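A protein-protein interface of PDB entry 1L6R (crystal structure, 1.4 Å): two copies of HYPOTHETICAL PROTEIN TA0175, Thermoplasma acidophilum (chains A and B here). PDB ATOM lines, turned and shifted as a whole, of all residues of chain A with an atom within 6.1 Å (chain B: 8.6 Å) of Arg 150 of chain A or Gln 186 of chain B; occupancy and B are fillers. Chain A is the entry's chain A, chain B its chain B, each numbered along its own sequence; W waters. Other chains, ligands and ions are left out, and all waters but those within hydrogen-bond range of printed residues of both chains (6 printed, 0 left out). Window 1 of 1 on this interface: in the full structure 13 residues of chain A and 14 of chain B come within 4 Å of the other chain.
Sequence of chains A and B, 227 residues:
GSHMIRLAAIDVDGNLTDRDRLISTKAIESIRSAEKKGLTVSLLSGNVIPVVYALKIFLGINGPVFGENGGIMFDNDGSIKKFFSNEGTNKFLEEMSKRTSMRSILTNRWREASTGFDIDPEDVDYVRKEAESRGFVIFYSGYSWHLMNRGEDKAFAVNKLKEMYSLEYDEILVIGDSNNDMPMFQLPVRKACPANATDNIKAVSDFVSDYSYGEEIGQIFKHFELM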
ATOM      1  N   PHE A  84      19.778 -17.042  -6.941  1.00  0.00           N
ATOM      2  CA  PHE A  84      19.753 -18.081  -7.955  1.00  0.00           C
ATOM      3  C   PHE A  84      21.049 -17.992  -8.737  1.00  0.00           C
ATOM      4  O   PHE A  84      21.756 -16.987  -8.676  1.00  0.00           O
ATOM      5  CB  PHE A  84      18.572 -17.904  -8.922  1.00  0.00           C
ATOM      6  CG  PHE A  84      17.226 -17.938  -8.254  1.00  0.00           C
ATOM      7  CD1 PHE A  84      16.721 -16.812  -7.615  1.00  0.00           C
ATOM      8  CD2 PHE A  84      16.473 -19.105  -8.250  1.00  0.00           C
ATOM      9  CE1 PHE A  84      15.479 -16.850  -6.979  1.00  0.00           C
ATOM     10  CE2 PHE A  84      15.232 -19.152  -7.621  1.00  0.00           C
ATOM     11  CZ  PHE A  84      14.735 -18.023  -6.984  1.00  0.00           C
ATOM     12  N   GLU A 132      11.127 -24.587 -20.508  1.00  0.00           N
ATOM     13  CA  GLU A 132      10.277 -25.089 -19.445  1.00  0.00           C
ATOM     14  C   GLU A 132      10.578 -26.553 -19.132  1.00  0.00           C
ATOM     15  O   GLU A 132      10.424 -26.988 -17.992  1.00  0.00           O
ATOM     16  CB  GLU A 132       8.802 -24.872 -19.808  1.00  0.00           C
ATOM     17  CG  GLU A 132       8.499 -23.403 -20.101  1.00  0.00           C
ATOM     18  CD  GLU A 132       7.025 -23.065 -20.074  1.00  0.00           C
ATOM     19  OE1 GLU A 132       6.200 -23.965 -20.318  1.00  0.00           O
ATOM     20  OE2 GLU A 132       6.689 -21.887 -19.821  1.00  0.00           O
ATOM     21  N   GLY A 135      13.153 -26.566 -16.429  1.00  0.00           N
ATOM     22  CA  GLY A 135      12.918 -25.858 -15.181  1.00  0.00           C
ATOM     23  C   GLY A 135      13.072 -24.348 -15.252  1.00  0.00           C
ATOM     24  O   GLY A 135      13.163 -23.685 -14.213  1.00  0.00           O
ATOM     25  N   PHE A 136      13.103 -23.811 -16.468  1.00  0.00           N
ATOM     26  CA  PHE A 136      13.246 -22.369 -16.667  1.00  0.00           C
ATOM     27  C   PHE A 136      11.984 -21.798 -17.306  1.00  0.00           C
ATOM     28  O   PHE A 136      11.077 -22.529 -17.698  1.00  0.00           O
ATOM     29  CB  PHE A 136      14.422 -22.054 -17.606  1.00  0.00           C
ATOM     30  CG  PHE A 136      15.714 -22.737 -17.238  1.00  0.00           C
ATOM     31  CD1 PHE A 136      16.200 -22.694 -15.942  1.00  0.00           C
ATOM     32  CD2 PHE A 136      16.455 -23.406 -18.207  1.00  0.00           C
ATOM     33  CE1 PHE A 136      17.409 -23.311 -15.612  1.00  0.00           C
ATOM     34  CE2 PHE A 136      17.665 -24.024 -17.883  1.00  0.00           C
ATOM     35  CZ  PHE A 136      18.137 -23.974 -16.585  1.00  0.00           C
ATOM     36  N   VAL A 137      11.926 -20.473 -17.385  1.00  0.00           N
ATOM     37  CA  VAL A 137      10.829 -19.794 -18.062  1.00  0.00           C
ATOM     38  C   VAL A 137      11.443 -18.643 -18.845  1.00  0.00           C
ATOM     39  O   VAL A 137      12.572 -18.218 -18.563  1.00  0.00           O
ATOM     40  CB  VAL A 137       9.756 -19.216 -17.091  1.00  0.00           C
ATOM     41  CG1 VAL A 137       9.103 -20.346 -16.292  1.00  0.00           C
ATOM     42  CG2 VAL A 137      10.377 -18.195 -16.156  1.00  0.00           C
ATOM     43  N   MET A 148      14.894 -17.298 -17.034  1.00  0.00           N
ATOM     44  CA  MET A 148      14.891 -17.328 -15.586  1.00  0.00           C
ATOM     45  C   MET A 148      14.642 -18.701 -15.008  1.00  0.00           C
ATOM     46  O   MET A 148      14.029 -19.556 -15.649  1.00  0.00           O
ATOM     47  CB  MET A 148      13.767 -16.427 -15.062  1.00  0.00           C
ATOM     48  CG  MET A 148      13.690 -15.043 -15.672  1.00  0.00           C
ATOM     49  SD  MET A 148      15.165 -14.074 -15.358  1.00  0.00           S
ATOM     50  CE  MET A 148      15.287 -14.247 -13.579  1.00  0.00           C
ATOM     51  N   ASN A 149      15.100 -18.891 -13.776  1.00  0.00           N
ATOM     52  CA  ASN A 149      14.838 -20.123 -13.053  1.00  0.00           C
ATOM     53  C   ASN A 149      13.371 -19.987 -12.601  1.00  0.00           C
ATOM     54  O   ASN A 149      12.913 -18.880 -12.280  1.00  0.00           O
ATOM     55  CB  ASN A 149      15.765 -20.209 -11.837  1.00  0.00           C
ATOM     56  CG  ASN A 149      17.213 -20.478 -12.227  1.00  0.00           C
ATOM     57  OD1 ASN A 149      17.561 -21.599 -12.606  1.00  0.00           O
ATOM     58  ND2 ASN A 149      18.058 -19.453 -12.151  1.00  0.00           N
ATOM     59  N   ARG A 150      12.619 -21.082 -12.592  1.00  0.00           N
ATOM     60  CA  ARG A 150      11.220 -21.015 -12.167  1.00  0.00           C
ATOM     61  C   ARG A 150      11.144 -20.454 -10.743  1.00  0.00           C
ATOM     62  O   ARG A 150      11.841 -20.928  -9.846  1.00  0.00           O
ATOM     63  CB  ARG A 150      10.591 -22.415 -12.203  1.00  0.00           C
ATOM     64  CG  ARG A 150       9.189 -22.514 -11.598  1.00  0.00           C
ATOM     65  CD  ARG A 150       8.107 -21.893 -12.465  1.00  0.00           C
ATOM     66  NE  ARG A 150       7.946 -22.595 -13.736  1.00  0.00           N
ATOM     67  CZ  ARG A 150       6.865 -22.506 -14.507  1.00  0.00           C
ATOM     68  NH1 ARG A 150       5.838 -21.755 -14.141  1.00  0.00           N
ATOM     69  NH2 ARG A 150       6.821 -23.166 -15.657  1.00  0.00           N
ATOM     70  N   GLY A 151      10.309 -19.436 -10.547  1.00  0.00           N
ATOM     71  CA  GLY A 151      10.159 -18.836  -9.232  1.00  0.00           C
ATOM     72  C   GLY A 151      11.043 -17.628  -8.968  1.00  0.00           C
ATOM     73  O   GLY A 151      10.935 -16.989  -7.919  1.00  0.00           O
ATOM     74  N   GLU A 152      11.919 -17.309  -9.914  1.00  0.00           N
ATOM     75  CA  GLU A 152      12.834 -16.176  -9.789  1.00  0.00           C
ATOM     76  C   GLU A 152      12.088 -15.010 -10.435  1.00  0.00           C
ATOM     77  O   GLU A 152      12.280 -14.688 -11.611  1.00  0.00           O
ATOM     78  CB  GLU A 152      14.127 -16.521 -10.529  1.00  0.00           C
ATOM     79  CG  GLU A 152      15.246 -15.519 -10.389  1.00  0.00           C
ATOM     80  CD  GLU A 152      16.518 -15.982 -11.084  1.00  0.00           C
ATOM     81  OE1 GLU A 152      16.480 -17.021 -11.782  1.00  0.00           O
ATOM     82  OE2 GLU A 152      17.559 -15.302 -10.937  1.00  0.00           O
ATOM     83  N   ASP A 153      11.231 -14.380  -9.643  1.00  0.00           N
ATOM     84  CA  ASP A 153      10.376 -13.321 -10.154  1.00  0.00           C
ATOM     85  C   ASP A 153      10.090 -12.205  -9.172  1.00  0.00           C
ATOM     86  O   ASP A 153      10.641 -12.169  -8.072  1.00  0.00           O
ATOM     87  CB  ASP A 153       9.048 -13.926 -10.630  1.00  0.00           C
ATOM     88  CG  ASP A 153       8.305 -14.682  -9.533  1.00  0.00           C
ATOM     89  OD1 ASP A 153       8.509 -14.396  -8.337  1.00  0.00           O
ATOM     90  OD2 ASP A 153       7.484 -15.566  -9.872  1.00  0.00           O
ATOM     91  N   PHE A 156       8.970 -13.232  -5.667  1.00  0.00           N
ATOM     92  CA  PHE A 156      10.076 -13.626  -4.807  1.00  0.00           C
ATOM     93  C   PHE A 156      10.685 -12.362  -4.180  1.00  0.00           C
ATOM     94  O   PHE A 156      10.940 -12.313  -2.978  1.00  0.00           O
ATOM     95  CB  PHE A 156      11.136 -14.365  -5.633  1.00  0.00           C
ATOM     96  CG  PHE A 156      12.389 -14.683  -4.872  1.00  0.00           C
ATOM     97  CD1 PHE A 156      12.506 -15.870  -4.153  1.00  0.00           C
ATOM     98  CD2 PHE A 156      13.454 -13.787  -4.860  1.00  0.00           C
ATOM     99  CE1 PHE A 156      13.668 -16.159  -3.429  1.00  0.00           C
ATOM    100  CE2 PHE A 156      14.621 -14.062  -4.140  1.00  0.00           C
ATOM    101  CZ  PHE A 156      14.729 -15.251  -3.422  1.00  0.00           C
ATOM    102  N   ASP B 153      -4.705 -18.878  -4.132  1.00  0.00           N
ATOM    103  CA  ASP B 153      -4.146 -20.141  -4.589  1.00  0.00           C
ATOM    104  C   ASP B 153      -3.303 -20.857  -3.554  1.00  0.00           C
ATOM    105  O   ASP B 153      -3.211 -20.425  -2.397  1.00  0.00           O
ATOM    106  CB  ASP B 153      -3.325 -19.915  -5.875  1.00  0.00           C
ATOM    107  CG  ASP B 153      -2.094 -19.035  -5.664  1.00  0.00           C
ATOM    108  OD1 ASP B 153      -1.664 -18.822  -4.511  1.00  0.00           O
ATOM    109  OD2 ASP B 153      -1.536 -18.559  -6.681  1.00  0.00           O
ATOM    110  N   ALA B 155      -0.080 -21.104  -3.274  1.00  0.00           N
ATOM    111  CA  ALA B 155       1.107 -20.398  -2.800  1.00  0.00           C
ATOM    112  C   ALA B 155       0.683 -19.482  -1.645  1.00  0.00           C
ATOM    113  O   ALA B 155       1.416 -19.301  -0.675  1.00  0.00           O
ATOM    114  CB  ALA B 155       1.743 -19.589  -3.924  1.00  0.00           C
ATOM    115  N   ASN B 159       2.420 -19.876   1.985  1.00  0.00           N
ATOM    116  CA  ASN B 159       3.041 -18.743   2.669  1.00  0.00           C
ATOM    117  C   ASN B 159       2.409 -18.564   4.046  1.00  0.00           C
ATOM    118  O   ASN B 159       3.093 -18.200   5.005  1.00  0.00           O
ATOM    119  CB  ASN B 159       2.924 -17.453   1.843  1.00  0.00           C
ATOM    120  CG  ASN B 159       3.954 -17.391   0.720  1.00  0.00           C
ATOM    121  OD1 ASN B 159       5.102 -17.796   0.899  1.00  0.00           O
ATOM    122  ND2 ASN B 159       3.554 -16.874  -0.434  1.00  0.00           N
ATOM    123  N   TYR B 169      11.558 -21.244   4.174  1.00  0.00           N
ATOM    124  CA  TYR B 169      11.071 -21.972   3.008  1.00  0.00           C
ATOM    125  C   TYR B 169      11.735 -23.341   2.827  1.00  0.00           C
ATOM    126  O   TYR B 169      11.091 -24.301   2.403  1.00  0.00           O
ATOM    127  CB  TYR B 169      11.293 -21.143   1.736  1.00  0.00           C
ATOM    128  CG  TYR B 169      10.294 -20.028   1.506  1.00  0.00           C
ATOM    129  CD1 TYR B 169       8.935 -20.300   1.354  1.00  0.00           C
ATOM    130  CD2 TYR B 169      10.721 -18.709   1.365  1.00  0.00           C
ATOM    131  CE1 TYR B 169       8.026 -19.291   1.059  1.00  0.00           C
ATOM    132  CE2 TYR B 169       9.821 -17.693   1.071  1.00  0.00           C
ATOM    133  CZ  TYR B 169       8.477 -17.991   0.913  1.00  0.00           C
ATOM    134  OH  TYR B 169       7.589 -16.994   0.575  1.00  0.00           O
ATOM    135  N   VAL B 174       6.754 -29.337  -0.599  1.00  0.00           N
ATOM    136  CA  VAL B 174       5.453 -29.309  -1.263  1.00  0.00           C
ATOM    137  C   VAL B 174       5.373 -30.489  -2.215  1.00  0.00           C
ATOM    138  O   VAL B 174       6.374 -30.867  -2.846  1.00  0.00           O
ATOM    139  CB  VAL B 174       5.185 -27.988  -2.051  1.00  0.00           C
ATOM    140  CG1 VAL B 174       5.178 -26.815  -1.101  1.00  0.00           C
ATOM    141  CG2 VAL B 174       6.200 -27.802  -3.171  1.00  0.00           C
ATOM    142  N   ASN B 179      -1.162 -28.439 -13.096  1.00  0.00           N
ATOM    143  CA  ASN B 179      -0.874 -27.028 -13.311  1.00  0.00           C
ATOM    144  C   ASN B 179      -1.308 -26.109 -12.180  1.00  0.00           C
ATOM    145  O   ASN B 179      -0.623 -25.132 -11.883  1.00  0.00           O
ATOM    146  CB  ASN B 179      -1.473 -26.531 -14.631  1.00  0.00           C
ATOM    147  CG  ASN B 179      -1.188 -25.056 -14.868  1.00  0.00           C
ATOM    148  OD1 ASN B 179      -2.054 -24.200 -14.659  1.00  0.00           O
ATOM    149  ND2 ASN B 179       0.040 -24.748 -15.281  1.00  0.00           N
ATOM    150  N   ASP B 181      -1.084 -26.678  -9.244  1.00  0.00           N
ATOM    151  CA  ASP B 181      -0.205 -26.918  -8.104  1.00  0.00           C
ATOM    152  C   ASP B 181       1.110 -26.162  -8.308  1.00  0.00           C
ATOM    153  O   ASP B 181       1.879 -25.969  -7.366  1.00  0.00           O
ATOM    154  CB  ASP B 181       0.106 -28.407  -7.947  1.00  0.00           C
ATOM    155  CG  ASP B 181      -1.122 -29.224  -7.633  1.00  0.00           C
ATOM    156  OD1 ASP B 181      -2.014 -28.727  -6.913  1.00  0.00           O
ATOM    157  OD2 ASP B 181      -1.193 -30.378  -8.097  1.00  0.00           O
ATOM    158  N   MET B 182       1.358 -25.732  -9.543  1.00  0.00           N
ATOM    159  CA  MET B 182       2.587 -25.006  -9.861  1.00  0.00           C
ATOM    160  C   MET B 182       2.836 -23.786  -8.954  1.00  0.00           C
ATOM    161  O   MET B 182       3.992 -23.452  -8.665  1.00  0.00           O
ATOM    162  CB  MET B 182       2.579 -24.592 -11.339  1.00  0.00           C
ATOM    163  CG  MET B 182       3.832 -23.848 -11.787  1.00  0.00           C
ATOM    164  SD  MET B 182       5.392 -24.764 -11.574  1.00  0.00           S
ATOM    165  CE  MET B 182       5.455 -25.708 -13.109  1.00  0.00           C
ATOM    166  N   PRO B 183       1.770 -23.099  -8.495  1.00  0.00           N
ATOM    167  CA  PRO B 183       2.040 -21.948  -7.624  1.00  0.00           C
ATOM    168  C   PRO B 183       2.935 -22.314  -6.430  1.00  0.00           C
ATOM    169  O   PRO B 183       3.781 -21.522  -6.023  1.00  0.00           O
ATOM    170  CB  PRO B 183       0.640 -21.503  -7.202  1.00  0.00           C
ATOM    171  CG  PRO B 183      -0.158 -21.759  -8.453  1.00  0.00           C
ATOM    172  CD  PRO B 183       0.345 -23.141  -8.884  1.00  0.00           C
ATOM    173  N   MET B 184       2.758 -23.516  -5.878  1.00  0.00           N
ATOM    174  CA  MET B 184       3.579 -23.964  -4.757  1.00  0.00           C
ATOM    175  C   MET B 184       5.031 -24.161  -5.182  1.00  0.00           C
ATOM    176  O   MET B 184       5.957 -23.897  -4.411  1.00  0.00           O
ATOM    177  CB  MET B 184       3.068 -25.297  -4.197  1.00  0.00           C
ATOM    178  CG  MET B 184       1.663 -25.259  -3.629  1.00  0.00           C
ATOM    179  SD  MET B 184       1.321 -26.731  -2.636  1.00  0.00           S
ATOM    180  CE  MET B 184       1.292 -28.016  -3.892  1.00  0.00           C
ATOM    181  N   PHE B 185       5.212 -24.631  -6.411  1.00  0.00           N
ATOM    182  CA  PHE B 185       6.539 -24.902  -6.943  1.00  0.00           C
ATOM    183  C   PHE B 185       7.270 -23.639  -7.384  1.00  0.00           C
ATOM    184  O   PHE B 185       8.418 -23.694  -7.823  1.00  0.00           O
ATOM    185  CB  PHE B 185       6.435 -25.915  -8.092  1.00  0.00           C
ATOM    186  CG  PHE B 185       6.036 -27.300  -7.643  1.00  0.00           C
ATOM    187  CD1 PHE B 185       4.727 -27.583  -7.255  1.00  0.00           C
ATOM    188  CD2 PHE B 185       6.984 -28.316  -7.578  1.00  0.00           C
ATOM    189  CE1 PHE B 185       4.372 -28.861  -6.810  1.00  0.00           C
ATOM    190  CE2 PHE B 185       6.641 -29.595  -7.134  1.00  0.00           C
ATOM    191  CZ  PHE B 185       5.334 -29.871  -6.748  1.00  0.00           C
ATOM    192  N   GLN B 186       6.609 -22.498  -7.263  1.00  0.00           N
ATOM    193  CA  GLN B 186       7.264 -21.250  -7.615  1.00  0.00           C
ATOM    194  C   GLN B 186       7.836 -20.587  -6.371  1.00  0.00           C
ATOM    195  O   GLN B 186       8.432 -19.510  -6.445  1.00  0.00           O
ATOM    196  CB  GLN B 186       6.294 -20.334  -8.351  1.00  0.00           C
ATOM    197  CG  GLN B 186       6.117 -20.791  -9.777  1.00  0.00           C
ATOM    198  CD  GLN B 186       5.176 -19.936 -10.585  1.00  0.00           C
ATOM    199  OE1 GLN B 186       5.008 -20.161 -11.782  1.00  0.00           O
ATOM    200  NE2 GLN B 186       4.551 -18.953  -9.942  1.00  0.00           N
ATOM    201  N   LEU B 187       7.653 -21.239  -5.224  1.00  0.00           N
ATOM    202  CA  LEU B 187       8.193 -20.732  -3.961  1.00  0.00           C
ATOM    203  C   LEU B 187       9.555 -21.385  -3.750  1.00  0.00           C
ATOM    204  O   LEU B 187       9.837 -22.433  -4.329  1.00  0.00           O
ATOM    205  CB  LEU B 187       7.253 -21.077  -2.802  1.00  0.00           C
ATOM    206  CG  LEU B 187       5.851 -20.456  -2.873  1.00  0.00           C
ATOM    207  CD1 LEU B 187       5.019 -20.927  -1.692  1.00  0.00           C
ATOM    208  CD2 LEU B 187       5.954 -18.939  -2.873  1.00  0.00           C
ATOM    209  N   PRO B 188      10.424 -20.777  -2.922  1.00  0.00           N
ATOM    210  CA  PRO B 188      11.760 -21.347  -2.673  1.00  0.00           C
ATOM    211  C   PRO B 188      11.757 -22.538  -1.724  1.00  0.00           C
ATOM    212  O   PRO B 188      12.654 -22.675  -0.889  1.00  0.00           O
ATOM    213  CB  PRO B 188      12.549 -20.185  -2.065  1.00  0.00           C
ATOM    214  CG  PRO B 188      11.661 -18.987  -2.157  1.00  0.00           C
ATOM    215  CD  PRO B 188      10.254 -19.495  -2.222  1.00  0.00           C
ATOM    216  N   VAL B 189      10.750 -23.392  -1.856  1.00  0.00           N
ATOM    217  CA  VAL B 189      10.597 -24.559  -0.995  1.00  0.00           C
ATOM    218  C   VAL B 189      11.212 -25.820  -1.583  1.00  0.00           C
ATOM    219  O   VAL B 189      11.719 -25.812  -2.697  1.00  0.00           O
ATOM    220  CB  VAL B 189       9.101 -24.836  -0.744  1.00  0.00           C
ATOM    221  CG1 VAL B 189       8.483 -23.656  -0.018  1.00  0.00           C
ATOM    222  CG2 VAL B 189       8.382 -25.076  -2.080  1.00  0.00           C
ATOM    223  N   LYS B 191      10.757 -29.374  -3.214  1.00  0.00           N
ATOM    224  CA  LYS B 191       9.708 -29.826  -4.110  1.00  0.00           C
ATOM    225  C   LYS B 191       9.771 -31.283  -4.532  1.00  0.00           C
ATOM    226  O   LYS B 191      10.838 -31.787  -4.856  1.00  0.00           O
ATOM    227  CB  LYS B 191       9.745 -28.936  -5.353  1.00  0.00           C
ATOM    228  CG  LYS B 191       9.651 -27.440  -5.016  1.00  0.00           C
ATOM    229  CD  LYS B 191      10.225 -26.541  -6.118  1.00  0.00           C
ATOM    230  CE  LYS B 191      10.272 -25.086  -5.645  1.00  0.00           C
ATOM    231  NZ  LYS B 191      10.884 -24.145  -6.631  1.00  0.00           N
ATOM    232  N   THR B 198       2.930 -33.303 -14.277  1.00  0.00           N
ATOM    233  CA  THR B 198       3.179 -32.643 -15.557  1.00  0.00           C
ATOM    234  C   THR B 198       4.678 -32.526 -15.810  1.00  0.00           C
ATOM    235  O   THR B 198       5.478 -32.543 -14.876  1.00  0.00           O
ATOM    236  CB  THR B 198       2.587 -31.225 -15.593  1.00  0.00           C
ATOM    237  OG1 THR B 198       3.309 -30.385 -14.686  1.00  0.00           O
ATOM    238  CG2 THR B 198       1.118 -31.253 -15.213  1.00  0.00           C
ATOM    239  N   ASP B 199       5.059 -32.393 -17.076  1.00  0.00           N
ATOM    240  CA  ASP B 199       6.472 -32.258 -17.413  1.00  0.00           C
ATOM    241  C   ASP B 199       7.060 -31.017 -16.738  1.00  0.00           C
ATOM    242  O   ASP B 199       8.196 -31.043 -16.258  1.00  0.00           O
ATOM    243  CB  ASP B 199       6.654 -32.167 -18.936  1.00  0.00           C
ATOM    244  CG  ASP B 199       6.322 -33.471 -19.648  1.00  0.00           C
ATOM    245  OD1 ASP B 199       6.185 -33.452 -20.889  1.00  0.00           O
ATOM    246  OD2 ASP B 199       6.209 -34.517 -18.972  1.00  0.00           O
ATOM    247  N   ASN B 200       6.285 -29.935 -16.676  1.00  0.00           N
ATOM    248  CA  ASN B 200       6.786 -28.714 -16.053  1.00  0.00           C
ATOM    249  C   ASN B 200       7.007 -28.862 -14.554  1.00  0.00           C
ATOM    250  O   ASN B 200       7.975 -28.324 -14.016  1.00  0.00           O
ATOM    251  CB  ASN B 200       5.850 -27.536 -16.343  1.00  0.00           C
ATOM    252  CG  ASN B 200       6.114 -26.915 -17.704  1.00  0.00           C
ATOM    253  OD1 ASN B 200       6.910 -27.434 -18.490  1.00  0.00           O
ATOM    254  ND2 ASN B 200       5.444 -25.800 -17.990  1.00  0.00           N
ATOM    255  N   ILE B 201       6.122 -29.594 -13.879  1.00  0.00           N
ATOM    256  CA  ILE B 201       6.276 -29.814 -12.443  1.00  0.00           C
ATOM    257  C   ILE B 201       7.493 -30.721 -12.199  1.00  0.00           C
ATOM    258  O   ILE B 201       8.303 -30.468 -11.311  1.00  0.00           O
ATOM    259  CB  ILE B 201       5.008 -30.471 -11.829  1.00  0.00           C
ATOM    260  CG1 ILE B 201       3.857 -29.457 -11.767  1.00  0.00           C
ATOM    261  CG2 ILE B 201       5.331 -31.035 -10.448  1.00  0.00           C
ATOM    262  CD1 ILE B 201       4.079 -28.309 -10.805  1.00  0.00           C
ATOM    263  N   ALA B 203      10.114 -31.015 -14.021  1.00  0.00           N
ATOM    264  CA  ALA B 203      11.322 -30.251 -14.319  1.00  0.00           C
ATOM    265  C   ALA B 203      11.801 -29.314 -13.211  1.00  0.00           C
ATOM    266  O   ALA B 203      12.971 -28.933 -13.184  1.00  0.00           O
ATOM    267  CB  ALA B 203      11.130 -29.465 -15.620  1.00  0.00           C
ATOM    268  N   VAL B 204      10.909 -28.939 -12.299  1.00  0.00           N
ATOM    269  CA  VAL B 204      11.306 -28.049 -11.217  1.00  0.00           C
ATOM    270  C   VAL B 204      11.349 -28.742  -9.857  1.00  0.00           C
ATOM    271  O   VAL B 204      11.719 -28.134  -8.858  1.00  0.00           O
ATOM    272  CB  VAL B 204      10.381 -26.805 -11.129  1.00  0.00           C
ATOM    273  CG1 VAL B 204      10.505 -25.984 -12.407  1.00  0.00           C
ATOM    274  CG2 VAL B 204       8.943 -27.223 -10.898  1.00  0.00           C
ATOM    275  N   SER B 205      10.993 -30.024  -9.823  1.00  0.00           N
ATOM    276  CA  SER B 205      11.003 -30.764  -8.566  1.00  0.00           C
ATOM    277  C   SER B 205      12.402 -31.198  -8.150  1.00  0.00           C
ATOM    278  O   SER B 205      13.263 -31.461  -8.998  1.00  0.00           O
ATOM    279  CB  SER B 205      10.112 -32.001  -8.674  1.00  0.00           C
ATOM    280  OG  SER B 205       8.745 -31.639  -8.766  1.00  0.00           O
HETATM  281  O   HOH W   1       9.159 -26.430 -15.770  1.00  0.00           O
HETATM  282  O   HOH W   2      11.853 -21.349  -6.996  1.00  0.00           O
HETATM  283  O   HOH W   3       5.453 -16.542  -8.309  1.00  0.00           O
HETATM  284  O   HOH W   4       6.423 -18.552 -13.929  1.00  0.00           O
HETATM  285  O   HOH W   5       7.683 -16.443  -6.523  1.00  0.00           O
HETATM  286  O   HOH W   6      10.889 -18.656  -5.661  1.00  0.00           O
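The guanidinium group (NH1) of Arg 150 of chain A is in hydrogen-bond range of the side-chain amide oxygen (OE1) of Gln 186 of chain B (3.0 Å). OE1 of Glu 132 of chain A sits at hydrogen-bond distance from ND2 of Asn 200 of chain B, 3.1 Å away.
The side-chain carboxylate (OD1) of Asp 153 of chain A is in hydrogen-bond range of the backbone NH (N) of Phe 156 of chain A (2.9 Å). O of Gly 135 of chain A lies within hydrogen-bond range of N of Arg 150 of chain A.
Among the printed residues, merely in contact across the chains: Glu 132 of chain A with Ala 203 of chain B (3.5 Å), Gly 135 of chain A with Ala 203 of chain B (3.6 Å), Gly 135 of chain A with Val 204 of chain B (3.7 Å), Arg 150 of chain A with Met 182 of chain B (3.7 Å), Arg 150 of chain A with Asn 200 of chain B (3.8 Å), Arg 150 of chain A with Val 204 of chain B (3.6 Å), Gly 151 of chain A with Gln 186 of chain B (3.3 Å) and Phe 156 of chain A with Pro 188 of chain B (3.7 Å).
Of chain B, only Met 182 (3.7 Å), Gln 186 (3.0 Å), Asn 200 (3.8 Å) and Val 204 (3.6 Å) come within 4 Å of Arg 150 of chain A. Of chain A, only Arg 150 (3.0 Å) and Gly 151 (3.3 Å) come within 4 Å of Gln 186 of chain B. Gly 151 of chain A touches just one residue of chain B: Gln 186. Of the printed residues of chain B, Gly 135 of chain A touches Ala 203 and Val 204. Of the printed residues of chain A, Pro 188 of chain B touches Phe 156 (3.7 Å). Tyr 169 of chain B touches none of the printed residues of chain A.
Water W1 bridges the backbone carbonyl oxygen of Glu 132 of chain A (2.6 Å) and the backbone carbonyl oxygen of Asn 200 of chain B (2.8 Å). Water W6 bridges O of Gln 186 of chain B (2.7 Å) and O of Gly 151 of chain A (2.8 Å). Water W3 lies within hydrogen-bond range of the side-chain carboxylate (OD2) of Asp 153 of chain A (2.7 Å) and the side-chain amide nitrogen (NE2) of Gln 186 of chain B (3.0 Å). Water W5 lies within hydrogen-bond range of OD1 of Asp 153 of chain A (2.9 Å) and O of Gln 186 of chain B (3.2 Å). Water W2 bridges O of Arg 150 of chain A (2.9 Å) and NZ of Lys 191 of chain B (3.0 Å). Water W4 lies within hydrogen-bond range of the side-chain amide oxygen of Gln 186 of chain B (3.0 Å) and the guanidinium group of Arg 150 of chain A (3.3 Å).
Position printed for both chains: 153.
Of the 23 printed residues of chain B, 6 touch a printed residue of chain A. Hydrophobic or aromatic side chains of chain B within 4 Å of the printed part of chain A: Met 182, Pro 188, Ala 203 and Val 204. Of the 12 printed residues of chain A, 5 touch a printed residue of chain B. Hydrophobic or aromatic side chains of chain A that line the printed part of chain B: Phe 156. Among the printed residues, 10 pairs touch across the chains. Among the printed residues, no Asp or Glu carboxylate lies within 4 Å of a Lys or Arg side-chain nitrogen of the other chain.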
